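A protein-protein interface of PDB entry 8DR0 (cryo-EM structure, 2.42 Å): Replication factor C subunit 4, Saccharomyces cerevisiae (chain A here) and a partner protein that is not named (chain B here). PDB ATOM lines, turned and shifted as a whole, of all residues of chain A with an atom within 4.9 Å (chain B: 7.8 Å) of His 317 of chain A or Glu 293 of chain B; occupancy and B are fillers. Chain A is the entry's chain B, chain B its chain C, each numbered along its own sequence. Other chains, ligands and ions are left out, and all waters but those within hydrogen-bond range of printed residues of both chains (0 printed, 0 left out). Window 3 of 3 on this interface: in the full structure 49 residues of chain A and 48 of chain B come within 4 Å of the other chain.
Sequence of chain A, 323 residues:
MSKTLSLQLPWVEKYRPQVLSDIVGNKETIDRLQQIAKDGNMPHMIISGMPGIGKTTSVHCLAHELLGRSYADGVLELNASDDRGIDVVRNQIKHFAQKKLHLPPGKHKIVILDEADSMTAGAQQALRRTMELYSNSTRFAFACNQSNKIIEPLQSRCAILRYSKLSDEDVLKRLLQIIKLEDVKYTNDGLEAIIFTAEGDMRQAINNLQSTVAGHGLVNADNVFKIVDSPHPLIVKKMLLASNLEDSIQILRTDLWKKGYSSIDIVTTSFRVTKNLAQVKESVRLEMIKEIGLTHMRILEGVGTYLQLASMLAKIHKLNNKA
The backbone carbonyl oxygen of His 317 of chain A sits close to the side-chain amide oxygen of Asn 321 of chain A (2.8 Å).
The guanidinium group (NH1) of Arg 296 of chain B is in salt-bridge range of the side-chain carboxylate (OE2) of Glu 246 of chain A, at 3.4 Å. A ring nitrogen (NE2) of His 317 of chain A lies close to the side-chain carboxylate (OE1) of Glu 293 of chain B (2.3 Å). The backbone NH (N) of Leu 245 of chain A sits at hydrogen-bond distance from the side-chain carboxylate (OE2) of Glu 293 of chain B (3.1 Å).
Of chain B, only Glu 293 comes within 4 Å of His 317 of chain A. Of the printed residues of chain A, Glu 293 of chain B touches Asn 244, Leu 245 and His 317. Of the printed residues of chain B, Asn 244 of chain A touches Glu 293 (3.8 Å). Of the printed residues of chain A, Arg 296 of chain B touches Glu 246. Of the printed residues of chain B, Glu 246 of chain A touches Arg 296. Of the printed residues of chain A, Val 297 of chain B touches Leu 245 (3.6 Å) and Lys 318 (3.9 Å). Asn 292 of chain B touches none of the printed residues of chain A. Ser 243 of chain A touches none of the printed residues of chain B. The nearest residue of chain B that does not touch His 317 of chain A is Val 297 of chain B (4.7 Å).
Hydrophobic or aromatic side chains of chain A within 4 Å of the printed part of chain B: Leu 245 and His 317. Among the printed residues, 6 pairs touch across the chains. Among the printed residues, Asp or Glu carboxylates within 4 Å of a Lys or Arg side-chain nitrogen of the other chain: Glu 246 of chain A with Arg 296 of chain B.
Glu 293 of chain B touches Asn 244 of chain A. CD2 of Leu 245 of chain A touches CG2 of Val 297 of chain B, 3.6 Å away. CG of Lys 318 of chain A touches CG1 of Val 297 of chain B (3.9 Å).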
ATOM      1  N   SER A 243       5.916  -4.694 -27.747  1.00  0.00           N
ATOM      2  CA  SER A 243       6.209  -5.190 -29.088  1.00  0.00           C
ATOM      3  C   SER A 243       6.754  -6.613 -29.051  1.00  0.00           C
ATOM      4  O   SER A 243       6.271  -7.489 -29.776  1.00  0.00           O
ATOM      5  CB  SER A 243       7.201  -4.256 -29.784  1.00  0.00           C
ATOM      6  OG  SER A 243       8.283  -3.936 -28.928  1.00  0.00           O
ATOM      7  N   ASN A 244       7.757  -6.860 -28.214  1.00  0.00           N
ATOM      8  CA  ASN A 244       8.389  -8.167 -28.109  1.00  0.00           C
ATOM      9  C   ASN A 244       7.804  -8.937 -26.933  1.00  0.00           C
ATOM     10  O   ASN A 244       7.520  -8.361 -25.878  1.00  0.00           O
ATOM     11  CB  ASN A 244       9.903  -8.027 -27.935  1.00  0.00           C
ATOM     12  CG  ASN A 244      10.566  -7.355 -29.120  1.00  0.00           C
ATOM     13  OD1 ASN A 244      10.335  -7.729 -30.271  1.00  0.00           O
ATOM     14  ND2 ASN A 244      11.398  -6.357 -28.847  1.00  0.00           N
ATOM     15  N   LEU A 245       7.624 -10.246 -27.122  1.00  0.00           N
ATOM     16  CA  LEU A 245       7.107 -11.079 -26.042  1.00  0.00           C
ATOM     17  C   LEU A 245       8.040 -11.067 -24.839  1.00  0.00           C
ATOM     18  O   LEU A 245       7.581 -11.185 -23.697  1.00  0.00           O
ATOM     19  CB  LEU A 245       6.896 -12.508 -26.541  1.00  0.00           C
ATOM     20  CG  LEU A 245       6.490 -13.546 -25.491  1.00  0.00           C
ATOM     21  CD1 LEU A 245       5.108 -13.235 -24.940  1.00  0.00           C
ATOM     22  CD2 LEU A 245       6.533 -14.944 -26.081  1.00  0.00           C
ATOM     23  N   GLU A 246       9.346 -10.930 -25.072  1.00  0.00           N
ATOM     24  CA  GLU A 246      10.294 -10.891 -23.964  1.00  0.00           C
ATOM     25  C   GLU A 246      10.033  -9.692 -23.061  1.00  0.00           C
ATOM     26  O   GLU A 246      10.082  -9.812 -21.832  1.00  0.00           O
ATOM     27  CB  GLU A 246      11.725 -10.857 -24.500  1.00  0.00           C
ATOM     28  CG  GLU A 246      12.112 -12.083 -25.312  1.00  0.00           C
ATOM     29  CD  GLU A 246      12.541 -13.249 -24.443  1.00  0.00           C
ATOM     30  OE1 GLU A 246      13.425 -13.055 -23.581  1.00  0.00           O
ATOM     31  OE2 GLU A 246      11.995 -14.358 -24.620  1.00  0.00           O
ATOM     32  N   LEU A 313       0.212 -14.467 -22.400  1.00  0.00           N
ATOM     33  CA  LEU A 313       0.951 -13.409 -23.081  1.00  0.00           C
ATOM     34  C   LEU A 313       1.504 -13.897 -24.415  1.00  0.00           C
ATOM     35  O   LEU A 313       1.475 -13.167 -25.411  1.00  0.00           O
ATOM     36  CB  LEU A 313       2.084 -12.896 -22.191  1.00  0.00           C
ATOM     37  CG  LEU A 313       1.690 -12.096 -20.947  1.00  0.00           C
ATOM     38  CD1 LEU A 313       2.931 -11.537 -20.269  1.00  0.00           C
ATOM     39  CD2 LEU A 313       0.722 -10.975 -21.291  1.00  0.00           C
ATOM     40  N   ALA A 314       2.018 -15.128 -24.450  1.00  0.00           N
ATOM     41  CA  ALA A 314       2.543 -15.671 -25.699  1.00  0.00           C
ATOM     42  C   ALA A 314       1.449 -15.789 -26.754  1.00  0.00           C
ATOM     43  O   ALA A 314       1.665 -15.461 -27.927  1.00  0.00           O
ATOM     44  CB  ALA A 314       3.194 -17.030 -25.447  1.00  0.00           C
ATOM     45  N   LYS A 315       0.267 -16.262 -26.356  1.00  0.00           N
ATOM     46  CA  LYS A 315      -0.831 -16.384 -27.309  1.00  0.00           C
ATOM     47  C   LYS A 315      -1.287 -15.016 -27.805  1.00  0.00           C
ATOM     48  O   LYS A 315      -1.598 -14.851 -28.991  1.00  0.00           O
ATOM     49  CB  LYS A 315      -1.993 -17.148 -26.676  1.00  0.00           C
ATOM     50  CG  LYS A 315      -1.678 -18.610 -26.404  1.00  0.00           C
ATOM     51  CD  LYS A 315      -2.919 -19.391 -26.017  1.00  0.00           C
ATOM     52  CE  LYS A 315      -2.586 -20.834 -25.681  1.00  0.00           C
ATOM     53  NZ  LYS A 315      -3.716 -21.523 -24.999  1.00  0.00           N
ATOM     54  N   ILE A 316      -1.330 -14.021 -26.916  1.00  0.00           N
ATOM     55  CA  ILE A 316      -1.682 -12.669 -27.346  1.00  0.00           C
ATOM     56  C   ILE A 316      -0.649 -12.145 -28.337  1.00  0.00           C
ATOM     57  O   ILE A 316      -0.996 -11.509 -29.341  1.00  0.00           O
ATOM     58  CB  ILE A 316      -1.823 -11.738 -26.127  1.00  0.00           C
ATOM     59  CG1 ILE A 316      -3.154 -11.997 -25.418  1.00  0.00           C
ATOM     60  CG2 ILE A 316      -1.720 -10.278 -26.555  1.00  0.00           C
ATOM     61  CD1 ILE A 316      -3.218 -11.436 -24.016  1.00  0.00           C
ATOM     62  N   HIS A 317       0.633 -12.393 -28.066  1.00  0.00           N
ATOM     63  CA  HIS A 317       1.682 -11.963 -28.984  1.00  0.00           C
ATOM     64  C   HIS A 317       1.527 -12.630 -30.344  1.00  0.00           C
ATOM     65  O   HIS A 317       1.700 -11.987 -31.385  1.00  0.00           O
ATOM     66  CB  HIS A 317       3.053 -12.273 -28.385  1.00  0.00           C
ATOM     67  CG  HIS A 317       4.201 -11.886 -29.263  1.00  0.00           C
ATOM     68  ND1 HIS A 317       4.763 -10.628 -29.240  1.00  0.00           N
ATOM     69  CD2 HIS A 317       4.901 -12.593 -30.181  1.00  0.00           C
ATOM     70  CE1 HIS A 317       5.755 -10.575 -30.110  1.00  0.00           C
ATOM     71  NE2 HIS A 317       5.860 -11.755 -30.695  1.00  0.00           N
ATOM     72  N   LYS A 318       1.201 -13.923 -30.354  1.00  0.00           N
ATOM     73  CA  LYS A 318       0.955 -14.611 -31.617  1.00  0.00           C
ATOM     74  C   LYS A 318      -0.217 -13.986 -32.361  1.00  0.00           C
ATOM     75  O   LYS A 318      -0.157 -13.792 -33.581  1.00  0.00           O
ATOM     76  CB  LYS A 318       0.692 -16.095 -31.368  1.00  0.00           C
ATOM     77  CG  LYS A 318       1.814 -17.012 -31.824  1.00  0.00           C
ATOM     78  CD  LYS A 318       1.338 -18.444 -32.061  1.00  0.00           C
ATOM     79  CE  LYS A 318       0.423 -18.953 -30.950  1.00  0.00           C
ATOM     80  NZ  LYS A 318      -0.065 -20.333 -31.226  1.00  0.00           N
ATOM     81  N   LEU A 319      -1.294 -13.664 -31.643  1.00  0.00           N
ATOM     82  CA  LEU A 319      -2.444 -13.031 -32.282  1.00  0.00           C
ATOM     83  C   LEU A 319      -2.065 -11.688 -32.892  1.00  0.00           C
ATOM     84  O   LEU A 319      -2.469 -11.371 -34.017  1.00  0.00           O
ATOM     85  CB  LEU A 319      -3.577 -12.851 -31.272  1.00  0.00           C
ATOM     86  CG  LEU A 319      -4.306 -14.117 -30.817  1.00  0.00           C
ATOM     87  CD1 LEU A 319      -5.234 -13.797 -29.656  1.00  0.00           C
ATOM     88  CD2 LEU A 319      -5.081 -14.738 -31.967  1.00  0.00           C
ATOM     89  N   ASN A 320      -1.287 -10.884 -32.165  1.00  0.00           N
ATOM     90  CA  ASN A 320      -0.933  -9.550 -32.636  1.00  0.00           C
ATOM     91  C   ASN A 320       0.076  -9.572 -33.776  1.00  0.00           C
ATOM     92  O   ASN A 320       0.318  -8.522 -34.382  1.00  0.00           O
ATOM     93  CB  ASN A 320      -0.380  -8.718 -31.478  1.00  0.00           C
ATOM     94  CG  ASN A 320      -1.467  -7.992 -30.711  1.00  0.00           C
ATOM     95  OD1 ASN A 320      -1.847  -8.399 -29.614  1.00  0.00           O
ATOM     96  ND2 ASN A 320      -1.976  -6.908 -31.288  1.00  0.00           N
ATOM     97  N   ASN A 321       0.667 -10.722 -34.081  1.00  0.00           N
ATOM     98  CA  ASN A 321       1.642 -10.817 -35.161  1.00  0.00           C
ATOM     99  C   ASN A 321       0.944 -10.918 -36.513  1.00  0.00           C
ATOM    100  O   ASN A 321       0.998 -11.955 -37.174  1.00  0.00           O
ATOM    101  CB  ASN A 321       2.560 -12.022 -34.952  1.00  0.00           C
ATOM    102  CG  ASN A 321       3.540 -11.817 -33.814  1.00  0.00           C
ATOM    103  OD1 ASN A 321       3.527 -10.783 -33.148  1.00  0.00           O
ATOM    104  ND2 ASN A 321       4.397 -12.806 -33.586  1.00  0.00           N
ATOM    105  N   LEU B 290      17.123 -17.320 -26.194  1.00  0.00           N
ATOM    106  CA  LEU B 290      16.628 -17.993 -27.385  1.00  0.00           C
ATOM    107  C   LEU B 290      16.644 -17.045 -28.575  1.00  0.00           C
ATOM    108  O   LEU B 290      16.218 -15.890 -28.471  1.00  0.00           O
ATOM    109  CB  LEU B 290      15.210 -18.523 -27.160  1.00  0.00           C
ATOM    110  CG  LEU B 290      15.004 -19.330 -25.876  1.00  0.00           C
ATOM    111  CD1 LEU B 290      13.529 -19.615 -25.654  1.00  0.00           C
ATOM    112  CD2 LEU B 290      15.802 -20.623 -25.918  1.00  0.00           C
ATOM    113  N   GLN B 291      17.141 -17.542 -29.709  1.00  0.00           N
ATOM    114  CA  GLN B 291      17.227 -16.714 -30.908  1.00  0.00           C
ATOM    115  C   GLN B 291      15.846 -16.421 -31.484  1.00  0.00           C
ATOM    116  O   GLN B 291      15.580 -15.299 -31.930  1.00  0.00           O
ATOM    117  CB  GLN B 291      18.106 -17.400 -31.954  1.00  0.00           C
ATOM    118  CG  GLN B 291      19.529 -17.677 -31.487  1.00  0.00           C
ATOM    119  CD  GLN B 291      20.074 -18.994 -32.011  1.00  0.00           C
ATOM    120  OE1 GLN B 291      20.779 -19.711 -31.301  1.00  0.00           O
ATOM    121  NE2 GLN B 291      19.757 -19.315 -33.260  1.00  0.00           N
ATOM    122  N   ASN B 292      14.958 -17.413 -31.485  1.00  0.00           N
ATOM    123  CA  ASN B 292      13.648 -17.302 -32.113  1.00  0.00           C
ATOM    124  C   ASN B 292      12.568 -17.225 -31.043  1.00  0.00           C
ATOM    125  O   ASN B 292      12.588 -17.996 -30.078  1.00  0.00           O
ATOM    126  CB  ASN B 292      13.391 -18.490 -33.042  1.00  0.00           C
ATOM    127  CG  ASN B 292      12.146 -18.312 -33.887  1.00  0.00           C
ATOM    128  OD1 ASN B 292      11.439 -17.311 -33.771  1.00  0.00           O
ATOM    129  ND2 ASN B 292      11.872 -19.285 -34.748  1.00  0.00           N
ATOM    130  N   GLU B 293      11.626 -16.295 -31.223  1.00  0.00           N
ATOM    131  CA  GLU B 293      10.540 -16.137 -30.260  1.00  0.00           C
ATOM    132  C   GLU B 293       9.531 -17.275 -30.357  1.00  0.00           C
ATOM    133  O   GLU B 293       8.854 -17.589 -29.368  1.00  0.00           O
ATOM    134  CB  GLU B 293       9.843 -14.794 -30.476  1.00  0.00           C
ATOM    135  CG  GLU B 293       9.609 -14.005 -29.201  1.00  0.00           C
ATOM    136  CD  GLU B 293       9.030 -12.629 -29.467  1.00  0.00           C
ATOM    137  OE1 GLU B 293       7.978 -12.545 -30.136  1.00  0.00           O
ATOM    138  OE2 GLU B 293       9.626 -11.632 -29.007  1.00  0.00           O
ATOM    139  N   GLU B 294       9.410 -17.895 -31.533  1.00  0.00           N
ATOM    140  CA  GLU B 294       8.479 -19.008 -31.689  1.00  0.00           C
ATOM    141  C   GLU B 294       8.813 -20.139 -30.727  1.00  0.00           C
ATOM    142  O   GLU B 294       7.914 -20.816 -30.218  1.00  0.00           O
ATOM    143  CB  GLU B 294       8.501 -19.509 -33.134  1.00  0.00           C
ATOM    144  CG  GLU B 294       7.525 -18.801 -34.063  1.00  0.00           C
ATOM    145  CD  GLU B 294       6.083 -18.935 -33.615  1.00  0.00           C
ATOM    146  OE1 GLU B 294       5.320 -17.958 -33.766  1.00  0.00           O
ATOM    147  OE2 GLU B 294       5.712 -20.016 -33.112  1.00  0.00           O
ATOM    148  N   THR B 295      10.104 -20.362 -30.472  1.00  0.00           N
ATOM    149  CA  THR B 295      10.501 -21.387 -29.513  1.00  0.00           C
ATOM    150  C   THR B 295       9.883 -21.121 -28.147  1.00  0.00           C
ATOM    151  O   THR B 295       9.268 -22.010 -27.546  1.00  0.00           O
ATOM    152  CB  THR B 295      12.027 -21.440 -29.411  1.00  0.00           C
ATOM    153  OG1 THR B 295      12.590 -21.654 -30.710  1.00  0.00           O
ATOM    154  CG2 THR B 295      12.467 -22.556 -28.475  1.00  0.00           C
ATOM    155  N   ARG B 296      10.036 -19.895 -27.642  1.00  0.00           N
ATOM    156  CA  ARG B 296       9.471 -19.554 -26.340  1.00  0.00           C
ATOM    157  C   ARG B 296       7.952 -19.651 -26.358  1.00  0.00           C
ATOM    158  O   ARG B 296       7.342 -20.132 -25.396  1.00  0.00           O
ATOM    159  CB  ARG B 296       9.911 -18.148 -25.931  1.00  0.00           C
ATOM    160  CG  ARG B 296       9.380 -17.706 -24.576  1.00  0.00           C
ATOM    161  CD  ARG B 296      10.477 -17.128 -23.697  1.00  0.00           C
ATOM    162  NE  ARG B 296      11.196 -18.169 -22.970  1.00  0.00           N
ATOM    163  CZ  ARG B 296      12.504 -18.172 -22.742  1.00  0.00           C
ATOM    164  NH1 ARG B 296      13.283 -17.184 -23.152  1.00  0.00           N
ATOM    165  NH2 ARG B 296      13.043 -19.192 -22.081  1.00  0.00           N
ATOM    166  N   VAL B 297       7.323 -19.189 -27.440  1.00  0.00           N
ATOM    167  CA  VAL B 297       5.865 -19.234 -27.520  1.00  0.00           C
ATOM    168  C   VAL B 297       5.374 -20.672 -27.405  1.00  0.00           C
ATOM    169  O   VAL B 297       4.482 -20.986 -26.604  1.00  0.00           O
ATOM    170  CB  VAL B 297       5.382 -18.578 -28.827  1.00  0.00           C
ATOM    171  CG1 VAL B 297       3.922 -18.917 -29.084  1.00  0.00           C
ATOM    172  CG2 VAL B 297       5.585 -17.074 -28.773  1.00  0.00           C
ATOM    173  N   HIS B 298       5.953 -21.569 -28.208  1.00  0.00           N
ATOM    174  CA  HIS B 298       5.531 -22.963 -28.185  1.00  0.00           C
ATOM    175  C   HIS B 298       5.827 -23.605 -26.837  1.00  0.00           C
ATOM    176  O   HIS B 298       4.989 -24.337 -26.294  1.00  0.00           O
ATOM    177  CB  HIS B 298       6.211 -23.737 -29.314  1.00  0.00           C
ATOM    178  CG  HIS B 298       5.703 -23.381 -30.676  1.00  0.00           C
ATOM    179  ND1 HIS B 298       4.434 -23.704 -31.104  1.00  0.00           N
ATOM    180  CD2 HIS B 298       6.293 -22.729 -31.707  1.00  0.00           C
ATOM    181  CE1 HIS B 298       4.263 -23.266 -32.338  1.00  0.00           C
ATOM    182  NE2 HIS B 298       5.376 -22.671 -32.728  1.00  0.00           N
ATOM    183  N   LEU B 299       7.011 -23.343 -26.274  1.00  0.00           N
ATOM    184  CA  LEU B 299       7.330 -23.880 -24.957  1.00  0.00           C
ATOM    185  C   LEU B 299       6.262 -23.490 -23.947  1.00  0.00           C
ATOM    186  O   LEU B 299       5.691 -24.347 -23.263  1.00  0.00           O
ATOM    187  CB  LEU B 299       8.697 -23.371 -24.495  1.00  0.00           C
ATOM    188  CG  LEU B 299       9.938 -24.047 -25.075  1.00  0.00           C
ATOM    189  CD1 LEU B 299      11.168 -23.188 -24.836  1.00  0.00           C
ATOM    190  CD2 LEU B 299      10.123 -25.433 -24.481  1.00  0.00           C
ATOM    191  N   LEU B 300       5.966 -22.192 -23.858  1.00  0.00           N
ATOM    192  CA  LEU B 300       5.029 -21.718 -22.849  1.00  0.00           C
ATOM    193  C   LEU B 300       3.647 -22.320 -23.063  1.00  0.00           C
ATOM    194  O   LEU B 300       3.034 -22.836 -22.123  1.00  0.00           O
ATOM    195  CB  LEU B 300       4.966 -20.191 -22.873  1.00  0.00           C
ATOM    196  CG  LEU B 300       6.240 -19.475 -22.418  1.00  0.00           C
ATOM    197  CD1 LEU B 300       6.152 -17.988 -22.726  1.00  0.00           C
ATOM    198  CD2 LEU B 300       6.498 -19.706 -20.937  1.00  0.00           C
ATOM    199  N   ASN B 333      13.098 -25.313 -33.498  1.00  0.00           N
ATOM    200  CA  ASN B 333      12.991 -24.062 -34.239  1.00  0.00           C
ATOM    201  C   ASN B 333      14.211 -23.164 -34.086  1.00  0.00           C
ATOM    202  O   ASN B 333      14.330 -22.183 -34.828  1.00  0.00           O
ATOM    203  CB  ASN B 333      11.747 -23.291 -33.792  1.00  0.00           C
ATOM    204  CG  ASN B 333      10.523 -24.175 -33.672  1.00  0.00           C
ATOM    205  OD1 ASN B 333      10.492 -25.286 -34.199  1.00  0.00           O
ATOM    206  ND2 ASN B 333       9.506 -23.685 -32.974  1.00  0.00           N
ATOM    207  N   GLU B 334      15.114 -23.464 -33.151  1.00  0.00           N
ATOM    208  CA  GLU B 334      16.268 -22.594 -32.944  1.00  0.00           C
ATOM    209  C   GLU B 334      17.272 -22.709 -34.083  1.00  0.00           C
ATOM    210  O   GLU B 334      18.035 -21.768 -34.329  1.00  0.00           O
ATOM    211  CB  GLU B 334      16.944 -22.924 -31.613  1.00  0.00           C
ATOM    212  CG  GLU B 334      16.178 -22.436 -30.394  1.00  0.00           C
ATOM    213  CD  GLU B 334      16.279 -20.935 -30.203  1.00  0.00           C
ATOM    214  OE1 GLU B 334      17.277 -20.474 -29.612  1.00  0.00           O
ATOM    215  OE2 GLU B 334      15.358 -20.216 -30.644  1.00  0.00           O
